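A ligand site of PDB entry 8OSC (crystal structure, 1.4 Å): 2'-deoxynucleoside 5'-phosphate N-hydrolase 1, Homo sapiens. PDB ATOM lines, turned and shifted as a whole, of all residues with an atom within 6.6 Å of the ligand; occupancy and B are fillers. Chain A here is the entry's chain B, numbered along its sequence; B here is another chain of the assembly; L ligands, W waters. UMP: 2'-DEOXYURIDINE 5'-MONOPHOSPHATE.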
ATOM      1  N   TYR A   7      16.660  -2.733  17.925  1.00  0.00           N
ATOM      2  CA  TYR A   7      17.915  -2.411  18.623  1.00  0.00           C
ATOM      3  C   TYR A   7      17.801  -2.927  20.057  1.00  0.00           C
ATOM      4  O   TYR A   7      16.870  -2.567  20.753  1.00  0.00           O
ATOM      5  CB  TYR A   7      18.119  -0.903  18.591  1.00  0.00           C
ATOM      6  CG  TYR A   7      19.419  -0.389  19.138  1.00  0.00           C
ATOM      7  CD1 TYR A   7      19.607  -0.247  20.505  1.00  0.00           C
ATOM      8  CD2 TYR A   7      20.442  -0.002  18.296  1.00  0.00           C
ATOM      9  CE1 TYR A   7      20.802   0.237  21.013  1.00  0.00           C
ATOM     10  CE2 TYR A   7      21.629   0.482  18.788  1.00  0.00           C
ATOM     11  CZ  TYR A   7      21.809   0.603  20.154  1.00  0.00           C
ATOM     12  OH  TYR A   7      22.993   1.091  20.622  1.00  0.00           O
ATOM     13  N   PHE A   8      18.756  -3.756  20.459  1.00  0.00           N
ATOM     14  CA  PHE A   8      18.783  -4.260  21.844  1.00  0.00           C
ATOM     15  C   PHE A   8      19.899  -3.607  22.663  1.00  0.00           C
ATOM     16  O   PHE A   8      21.027  -3.602  22.203  1.00  0.00           O
ATOM     17  CB  PHE A   8      18.892  -5.786  21.893  1.00  0.00           C
ATOM     18  CG  PHE A   8      18.993  -6.313  23.301  1.00  0.00           C
ATOM     19  CD1 PHE A   8      17.891  -6.337  24.127  1.00  0.00           C
ATOM     20  CD2 PHE A   8      20.210  -6.727  23.812  1.00  0.00           C
ATOM     21  CE1 PHE A   8      17.990  -6.800  25.433  1.00  0.00           C
ATOM     22  CE2 PHE A   8      20.309  -7.190  25.118  1.00  0.00           C
ATOM     23  CZ  PHE A   8      19.194  -7.231  25.918  1.00  0.00           C
ATOM     24  N   CYS A   9      19.542  -3.122  23.859  1.00  0.00           N
ATOM     25  CA  CYS A   9      20.502  -2.499  24.797  1.00  0.00           C
ATOM     26  C   CYS A   9      20.545  -3.305  26.113  1.00  0.00           C
ATOM     27  O   CYS A   9      19.496  -3.592  26.653  1.00  0.00           O
ATOM     28  CB  CYS A   9      20.102  -1.095  25.252  1.00  0.00           C
ATOM     29  SG  CYS A   9      19.181  -0.009  24.134  1.00  0.00           S
ATOM     30  N   GLY A  10      21.739  -3.621  26.577  1.00  0.00           N
ATOM     31  CA  GLY A  10      21.922  -4.275  27.876  1.00  0.00           C
ATOM     32  C   GLY A  10      23.279  -3.925  28.442  1.00  0.00           C
ATOM     33  O   GLY A  10      24.160  -3.608  27.681  1.00  0.00           O
ATOM     34  N   SER A  11      23.431  -4.011  29.765  1.00  0.00           N
ATOM     35  CA  SER A  11      24.692  -3.620  30.427  1.00  0.00           C
ATOM     36  C   SER A  11      25.881  -4.418  29.938  1.00  0.00           C
ATOM     37  O   SER A  11      25.751  -5.629  29.753  1.00  0.00           O
ATOM     38  CB  SER A  11      24.590  -3.728  31.922  1.00  0.00           C
ATOM     39  OG  SER A  11      25.823  -3.447  32.541  1.00  0.00           O
ATOM     40  N   ILE A  12      26.996  -3.734  29.721  1.00  0.00           N
ATOM     41  CA  ILE A  12      28.267  -4.437  29.390  1.00  0.00           C
ATOM     42  C   ILE A  12      29.305  -3.980  30.440  1.00  0.00           C
ATOM     43  O   ILE A  12      29.547  -4.721  31.385  1.00  0.00           O
ATOM     44  CB  ILE A  12      28.708  -4.171  27.950  1.00  0.00           C
ATOM     45  CG1 ILE A  12      27.671  -4.673  26.952  1.00  0.00           C
ATOM     46  CG2 ILE A  12      30.083  -4.755  27.690  1.00  0.00           C
ATOM     47  CD1 ILE A  12      28.037  -4.453  25.503  1.00  0.00           C
ATOM     48  N   ARG A  13      29.831  -2.773  30.289  1.00  0.00           N
ATOM     49  CA  ARG A  13      30.832  -2.247  31.246  1.00  0.00           C
ATOM     50  C   ARG A  13      30.180  -1.951  32.610  1.00  0.00           C
ATOM     51  O   ARG A  13      30.904  -1.832  33.588  1.00  0.00           O
ATOM     52  CB  ARG A  13      31.548  -1.041  30.640  1.00  0.00           C
ATOM     53  CG  ARG A  13      32.384  -1.379  29.414  1.00  0.00           C
ATOM     54  CD  ARG A  13      33.344  -0.285  29.024  1.00  0.00           C
ATOM     55  NE  ARG A  13      34.068  -0.657  27.826  1.00  0.00           N
ATOM     56  CZ  ARG A  13      34.728   0.185  27.051  1.00  0.00           C
ATOM     57  NH1 ARG A  13      34.765   1.469  27.337  1.00  0.00           N
ATOM     58  NH2 ARG A  13      35.363  -0.264  25.978  1.00  0.00           N
ATOM     59  N   GLY A  14      28.860  -1.854  32.668  1.00  0.00           N
ATOM     60  CA  GLY A  14      28.204  -1.689  33.990  1.00  0.00           C
ATOM     61  C   GLY A  14      28.071  -3.009  34.716  1.00  0.00           C
ATOM     62  O   GLY A  14      27.718  -2.994  35.900  1.00  0.00           O
ATOM     63  N   GLY A  15      28.354  -4.125  34.033  1.00  0.00           N
ATOM     64  CA  GLY A  15      28.191  -5.467  34.614  1.00  0.00           C
ATOM     65  C   GLY A  15      27.582  -6.451  33.639  1.00  0.00           C
ATOM     66  O   GLY A  15      26.608  -6.098  32.994  1.00  0.00           O
ATOM     67  N   THR A  37      21.885  -4.928  16.657  1.00  0.00           N
ATOM     68  CA  THR A  37      23.002  -4.916  17.621  1.00  0.00           C
ATOM     69  C   THR A  37      23.735  -6.266  17.699  1.00  0.00           C
ATOM     70  O   THR A  37      24.842  -6.260  18.233  1.00  0.00           O
ATOM     71  CB  THR A  37      22.461  -4.472  18.988  1.00  0.00           C
ATOM     72  OG1 THR A  37      21.192  -5.084  19.181  1.00  0.00           O
ATOM     73  CG2 THR A  37      22.316  -2.974  19.077  1.00  0.00           C
ATOM     74  N   ASP A  56      36.369   3.303  21.628  1.00  0.00           N
ATOM     75  CA  ASP A  56      35.124   3.763  22.275  1.00  0.00           C
ATOM     76  C   ASP A  56      34.325   4.667  21.330  1.00  0.00           C
ATOM     77  O   ASP A  56      33.131   4.520  21.255  1.00  0.00           O
ATOM     78  CB  ASP A  56      35.417   4.367  23.652  1.00  0.00           C
ATOM     79  CG  ASP A  56      35.793   3.329  24.696  1.00  0.00           C
ATOM     80  OD1 ASP A  56      35.692   2.139  24.390  1.00  0.00           O
ATOM     81  OD2 ASP A  56      36.175   3.729  25.797  1.00  0.00           O
ATOM     82  N   ILE A  59      32.597   2.484  18.781  1.00  0.00           N
ATOM     83  CA  ILE A  59      31.415   1.805  19.369  1.00  0.00           C
ATOM     84  C   ILE A  59      30.268   2.822  19.453  1.00  0.00           C
ATOM     85  O   ILE A  59      29.163   2.498  19.054  1.00  0.00           O
ATOM     86  CB  ILE A  59      31.777   1.242  20.748  1.00  0.00           C
ATOM     87  CG1 ILE A  59      32.714   0.040  20.632  1.00  0.00           C
ATOM     88  CG2 ILE A  59      30.529   0.903  21.544  1.00  0.00           C
ATOM     89  CD1 ILE A  59      33.419  -0.317  21.910  1.00  0.00           C
ATOM     90  N   ASP A  63      26.806   2.441  17.293  1.00  0.00           N
ATOM     91  CA  ASP A  63      25.574   2.241  18.092  1.00  0.00           C
ATOM     92  C   ASP A  63      24.568   3.338  17.751  1.00  0.00           C
ATOM     93  O   ASP A  63      23.397   3.032  17.607  1.00  0.00           O
ATOM     94  CB  ASP A  63      25.906   2.144  19.578  1.00  0.00           C
ATOM     95  CG  ASP A  63      26.545   0.831  19.969  1.00  0.00           C
ATOM     96  OD1 ASP A  63      26.660  -0.034  19.102  1.00  0.00           O
ATOM     97  OD2 ASP A  63      26.914   0.692  21.137  1.00  0.00           O
ATOM     98  N   PRO A  80      22.238  -1.600  36.510  1.00  0.00           N
ATOM     99  CA  PRO A  80      22.537  -0.182  36.248  1.00  0.00           C
ATOM    100  C   PRO A  80      23.682  -0.036  35.248  1.00  0.00           C
ATOM    101  O   PRO A  80      24.700  -0.727  35.324  1.00  0.00           O
ATOM    102  CB  PRO A  80      22.933   0.353  37.628  1.00  0.00           C
ATOM    103  CG  PRO A  80      22.192  -0.562  38.595  1.00  0.00           C
ATOM    104  CD  PRO A  80      22.294  -1.907  37.957  1.00  0.00           C
ATOM    105  N   SER A  81      23.510   0.889  34.305  1.00  0.00           N
ATOM    106  CA  SER A  81      24.463   1.025  33.198  1.00  0.00           C
ATOM    107  C   SER A  81      24.367   2.422  32.632  1.00  0.00           C
ATOM    108  O   SER A  81      23.282   2.858  32.217  1.00  0.00           O
ATOM    109  CB  SER A  81      24.095   0.009  32.102  1.00  0.00           C
ATOM    110  OG  SER A  81      24.790   0.331  30.918  1.00  0.00           O
ATOM    111  N   LEU A  82      25.504   3.120  32.577  1.00  0.00           N
ATOM    112  CA  LEU A  82      25.532   4.427  31.940  1.00  0.00           C
ATOM    113  C   LEU A  82      25.182   4.316  30.464  1.00  0.00           C
ATOM    114  O   LEU A  82      24.474   5.170  29.924  1.00  0.00           O
ATOM    115  CB  LEU A  82      26.924   5.038  32.058  1.00  0.00           C
ATOM    116  CG  LEU A  82      27.326   5.516  33.449  1.00  0.00           C
ATOM    117  CD1 LEU A  82      28.824   5.768  33.489  1.00  0.00           C
ATOM    118  CD2 LEU A  82      26.597   6.751  33.921  1.00  0.00           C
ATOM    119  N   GLY A  83      25.708   3.276  29.799  1.00  0.00           N
ATOM    120  CA  GLY A  83      25.520   3.149  28.368  1.00  0.00           C
ATOM    121  C   GLY A  83      24.091   2.868  27.995  1.00  0.00           C
ATOM    122  O   GLY A  83      23.572   3.440  27.042  1.00  0.00           O
ATOM    123  N   VAL A  84      23.412   1.997  28.748  1.00  0.00           N
ATOM    124  CA  VAL A  84      22.008   1.729  28.478  1.00  0.00           C
ATOM    125  C   VAL A  84      21.175   2.986  28.731  1.00  0.00           C
ATOM    126  O   VAL A  84      20.301   3.332  27.935  1.00  0.00           O
ATOM    127  CB  VAL A  84      21.514   0.554  29.337  1.00  0.00           C
ATOM    128  CG1 VAL A  84      20.011   0.400  29.222  1.00  0.00           C
ATOM    129  CG2 VAL A  84      22.227  -0.729  28.930  1.00  0.00           C
ATOM    130  N   GLY A  85      21.451   3.700  29.828  1.00  0.00           N
ATOM    131  CA  GLY A  85      20.725   4.941  30.074  1.00  0.00           C
ATOM    132  C   GLY A  85      20.946   5.950  28.970  1.00  0.00           C
ATOM    133  O   GLY A  85      19.994   6.594  28.490  1.00  0.00           O
ATOM    134  N   GLU A  87      21.798   5.378  25.787  1.00  0.00           N
ATOM    135  CA  GLU A  87      21.088   4.943  24.587  1.00  0.00           C
ATOM    136  C   GLU A  87      19.600   5.247  24.705  1.00  0.00           C
ATOM    137  O   GLU A  87      18.969   5.683  23.729  1.00  0.00           O
ATOM    138  CB  GLU A  87      21.315   3.449  24.357  1.00  0.00           C
ATOM    139  CG  GLU A  87      22.729   3.097  23.903  1.00  0.00           C
ATOM    140  CD  GLU A  87      22.972   1.584  23.889  1.00  0.00           C
ATOM    141  OE1 GLU A  87      23.553   1.085  22.900  1.00  0.00           O
ATOM    142  OE2 GLU A  87      22.607   0.888  24.875  1.00  0.00           O
ATOM    143  N   PRO B  80      28.201   3.342  37.782  1.00  0.00           N
ATOM    144  CA  PRO B  80      27.225   3.073  36.733  1.00  0.00           C
ATOM    145  C   PRO B  80      25.795   3.441  37.187  1.00  0.00           C
ATOM    146  O   PRO B  80      25.413   3.113  38.273  1.00  0.00           O
ATOM    147  CB  PRO B  80      27.397   1.567  36.471  1.00  0.00           C
ATOM    148  CG  PRO B  80      28.810   1.280  36.920  1.00  0.00           C
ATOM    149  CD  PRO B  80      29.007   2.177  38.130  1.00  0.00           C
ATOM    150  N   VAL B 109      36.188   0.355  34.213  1.00  0.00           N
ATOM    151  CA  VAL B 109      36.366   0.885  32.865  1.00  0.00           C
ATOM    152  C   VAL B 109      35.099   1.650  32.515  1.00  0.00           C
ATOM    153  O   VAL B 109      33.999   1.100  32.551  1.00  0.00           O
ATOM    154  CB  VAL B 109      36.606  -0.237  31.845  1.00  0.00           C
ATOM    155  CG1 VAL B 109      37.013   0.356  30.502  1.00  0.00           C
ATOM    156  CG2 VAL B 109      37.670  -1.219  32.344  1.00  0.00           C
ATOM    157  N   LEU B 110      35.250   2.936  32.203  1.00  0.00           N
ATOM    158  CA  LEU B 110      34.095   3.768  31.890  1.00  0.00           C
ATOM    159  C   LEU B 110      33.404   3.300  30.599  1.00  0.00           C
ATOM    160  O   LEU B 110      34.061   2.953  29.623  1.00  0.00           O
ATOM    161  CB  LEU B 110      34.508   5.231  31.752  1.00  0.00           C
ATOM    162  CG  LEU B 110      33.424   6.210  31.327  1.00  0.00           C
ATOM    163  CD1 LEU B 110      32.322   6.256  32.369  1.00  0.00           C
ATOM    164  CD2 LEU B 110      34.006   7.609  31.115  1.00  0.00           C
ATOM    165  N   SER B 111      32.075   3.291  30.637  1.00  0.00           N
ATOM    166  CA  SER B 111      31.224   2.928  29.504  1.00  0.00           C
ATOM    167  C   SER B 111      31.738   3.534  28.205  1.00  0.00           C
ATOM    168  O   SER B 111      32.041   4.736  28.128  1.00  0.00           O
ATOM    169  CB  SER B 111      29.821   3.479  29.771  1.00  0.00           C
ATOM    170  OG  SER B 111      28.976   3.346  28.620  1.00  0.00           O
ATOM    171  N   ALA B 112      31.800   2.701  27.159  1.00  0.00           N
ATOM    172  CA  ALA B 112      32.234   3.200  25.855  1.00  0.00           C
ATOM    173  C   ALA B 112      31.264   4.232  25.292  1.00  0.00           C
ATOM    174  O   ALA B 112      31.666   5.088  24.499  1.00  0.00           O
ATOM    175  CB  ALA B 112      32.395   2.045  24.866  1.00  0.00           C
ATOM    176  N   MET B 113      29.993   4.205  25.699  1.00  0.00           N
ATOM    177  CA  MET B 113      29.064   5.188  25.155  1.00  0.00           C
ATOM    178  C   MET B 113      29.347   6.568  25.713  1.00  0.00           C
ATOM    179  O   MET B 113      29.078   7.584  25.059  1.00  0.00           O
ATOM    180  CB  MET B 113      27.614   4.816  25.478  1.00  0.00           C
ATOM    181  CG  MET B 113      27.293   3.496  24.823  1.00  0.00           C
ATOM    182  SD  MET B 113      27.345   3.578  23.026  1.00  0.00           S
ATOM    183  CE  MET B 113      26.175   4.854  22.671  1.00  0.00           C
ATOM    184  N   ILE B 114      29.879   6.643  26.930  1.00  0.00           N
ATOM    185  CA  ILE B 114      30.243   7.926  27.526  1.00  0.00           C
ATOM    186  C   ILE B 114      31.627   8.358  27.082  1.00  0.00           C
ATOM    187  O   ILE B 114      31.814   9.472  26.581  1.00  0.00           O
ATOM    188  CB  ILE B 114      30.115   7.859  29.065  1.00  0.00           C
ATOM    189  CG1 ILE B 114      28.696   7.402  29.469  1.00  0.00           C
ATOM    190  CG2 ILE B 114      30.486   9.215  29.677  1.00  0.00           C
ATOM    191  CD1 ILE B 114      27.591   8.253  28.851  1.00  0.00           C
HETATM  192  N1  UMP L   1      27.950  -0.481  24.503  1.00  0.00           N
HETATM  193  C2  UMP L   1      28.788   0.112  25.429  1.00  0.00           C
HETATM  194  N3  UMP L   1      30.063  -0.401  25.472  1.00  0.00           N
HETATM  195  C4  UMP L   1      30.574  -1.414  24.693  1.00  0.00           C
HETATM  196  C5  UMP L   1      29.648  -1.967  23.745  1.00  0.00           C
HETATM  197  C6  UMP L   1      28.404  -1.490  23.687  1.00  0.00           C
HETATM  198  O2  UMP L   1      28.450   1.020  26.177  1.00  0.00           O
HETATM  199  O4  UMP L   1      31.740  -1.760  24.851  1.00  0.00           O
HETATM  200  C1' UMP L   1      26.548  -0.002  24.361  1.00  0.00           C
HETATM  201  C2' UMP L   1      25.574  -1.109  23.964  1.00  0.00           C
HETATM  202  C3' UMP L   1      24.961  -1.568  25.288  1.00  0.00           C
HETATM  203  C4' UMP L   1      25.326  -0.483  26.296  1.00  0.00           C
HETATM  204  O3' UMP L   1      23.547  -1.656  25.163  1.00  0.00           O
HETATM  205  O4' UMP L   1      26.079   0.523  25.584  1.00  0.00           O
HETATM  206  C5' UMP L   1      26.127  -0.954  27.478  1.00  0.00           C
HETATM  207  O5' UMP L   1      26.673   0.196  28.143  1.00  0.00           O
HETATM  208  P   UMP L   1      27.688  -0.024  29.369  1.00  0.00           P
HETATM  209  OP1 UMP L   1      28.952  -0.553  28.745  1.00  0.00           O
HETATM  210  OP2 UMP L   1      27.860   1.328  30.005  1.00  0.00           O
HETATM  211  OP3 UMP L   1      27.015  -1.008  30.298  1.00  0.00           O
HETATM  212  O   HOH W   1      28.088   1.710  32.791  1.00  0.00           O
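The side-chain hydroxyl of Ser 81 lies within hydrogen-bond range of an oxygen (OP3) of the ligand, 2.7 Å away.
The side-chain hydroxyl (OG) of Ser 111 of chain B sits at hydrogen-bond distance from an oxygen (OP2) of the ligand.
The side-chain carboxylate (OE2) of Glu 87 is in hydrogen-bond range of an oxygen (O3') of the ligand.
OP3 of the ligand sits at hydrogen-bond distance from N of Ile 12.
N of Arg 13 lies within hydrogen-bond range of OP1 of the ligand, at 2.8 Å.
N of Gly 83 sits at hydrogen-bond distance from OP2 of the ligand, at 2.9 Å.
An oxygen (O3') of the ligand is in hydrogen-bond range of the backbone NH of Gly 10.
O of Gly 10 lies within hydrogen-bond range of O3' of the ligand (3.2 Å).
An oxygen (OP3) of the ligand is in hydrogen-bond range of the backbone NH (N) of Gly 14 (3.1 Å).
The side-chain hydroxyl of Ser 81 sits close to the backbone NH of Gly 83 (3.3 Å).
OG of Ser 81 is in hydrogen-bond range of N of Val 84 (3.1 Å).
N of Gly 83 lies close to OG of Ser 111 of chain B, at 3.5 Å.
OG of Ser 111 of chain B lies close to N of Met 113 of chain B (3.2 Å).
The side-chain carboxylate of Asp 56 lies within salt-bridge range of the guanidinium group of Arg 13 (2.9 Å).
NH1 of Arg 13 sits at hydrogen-bond distance from O of Leu 110 of chain B (2.8 Å).
The side-chain hydroxyl (OG) of Ser 11 lies close to the backbone NH (N) of Gly 14 (3.4 Å).
OG of Ser 11 sits at hydrogen-bond distance from O of Gly 15.
Cys 9 touches the ligand (CA to O3', 3.2 Å).
Ser 11 touches the ligand (CA to OP3, 3.5 Å).
CD1 of Ile 59 touches O4 of the ligand (3.7 Å).
Asp 63 touches the ligand (OD2 to C1', 3.3 Å).
N of Leu 82 touches OP2 of the ligand, 3.9 Å away.
Val 84 touches the ligand (N to O5', 3.8 Å).
Ala 112 of chain B touches the ligand.
Met 113 of chain B touches the ligand (CG to O2, 3.1 Å).
Hydrophobic or aromatic side chains within 4 Å of the ligand: Ile 12, Ile 59, Ala 112 of chain B and Met 113 of chain B.
Of the 27 residues printed, 16 come within 4 Å of the ligand.
The nearest printed residue that does not touch the ligand is Phe 8 (4.3 Å).
Water W1 lies within hydrogen-bond range of an oxygen (OP2) of the ligand (2.8 Å) and the backbone NH (N) of Leu 82 (3.0 Å).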
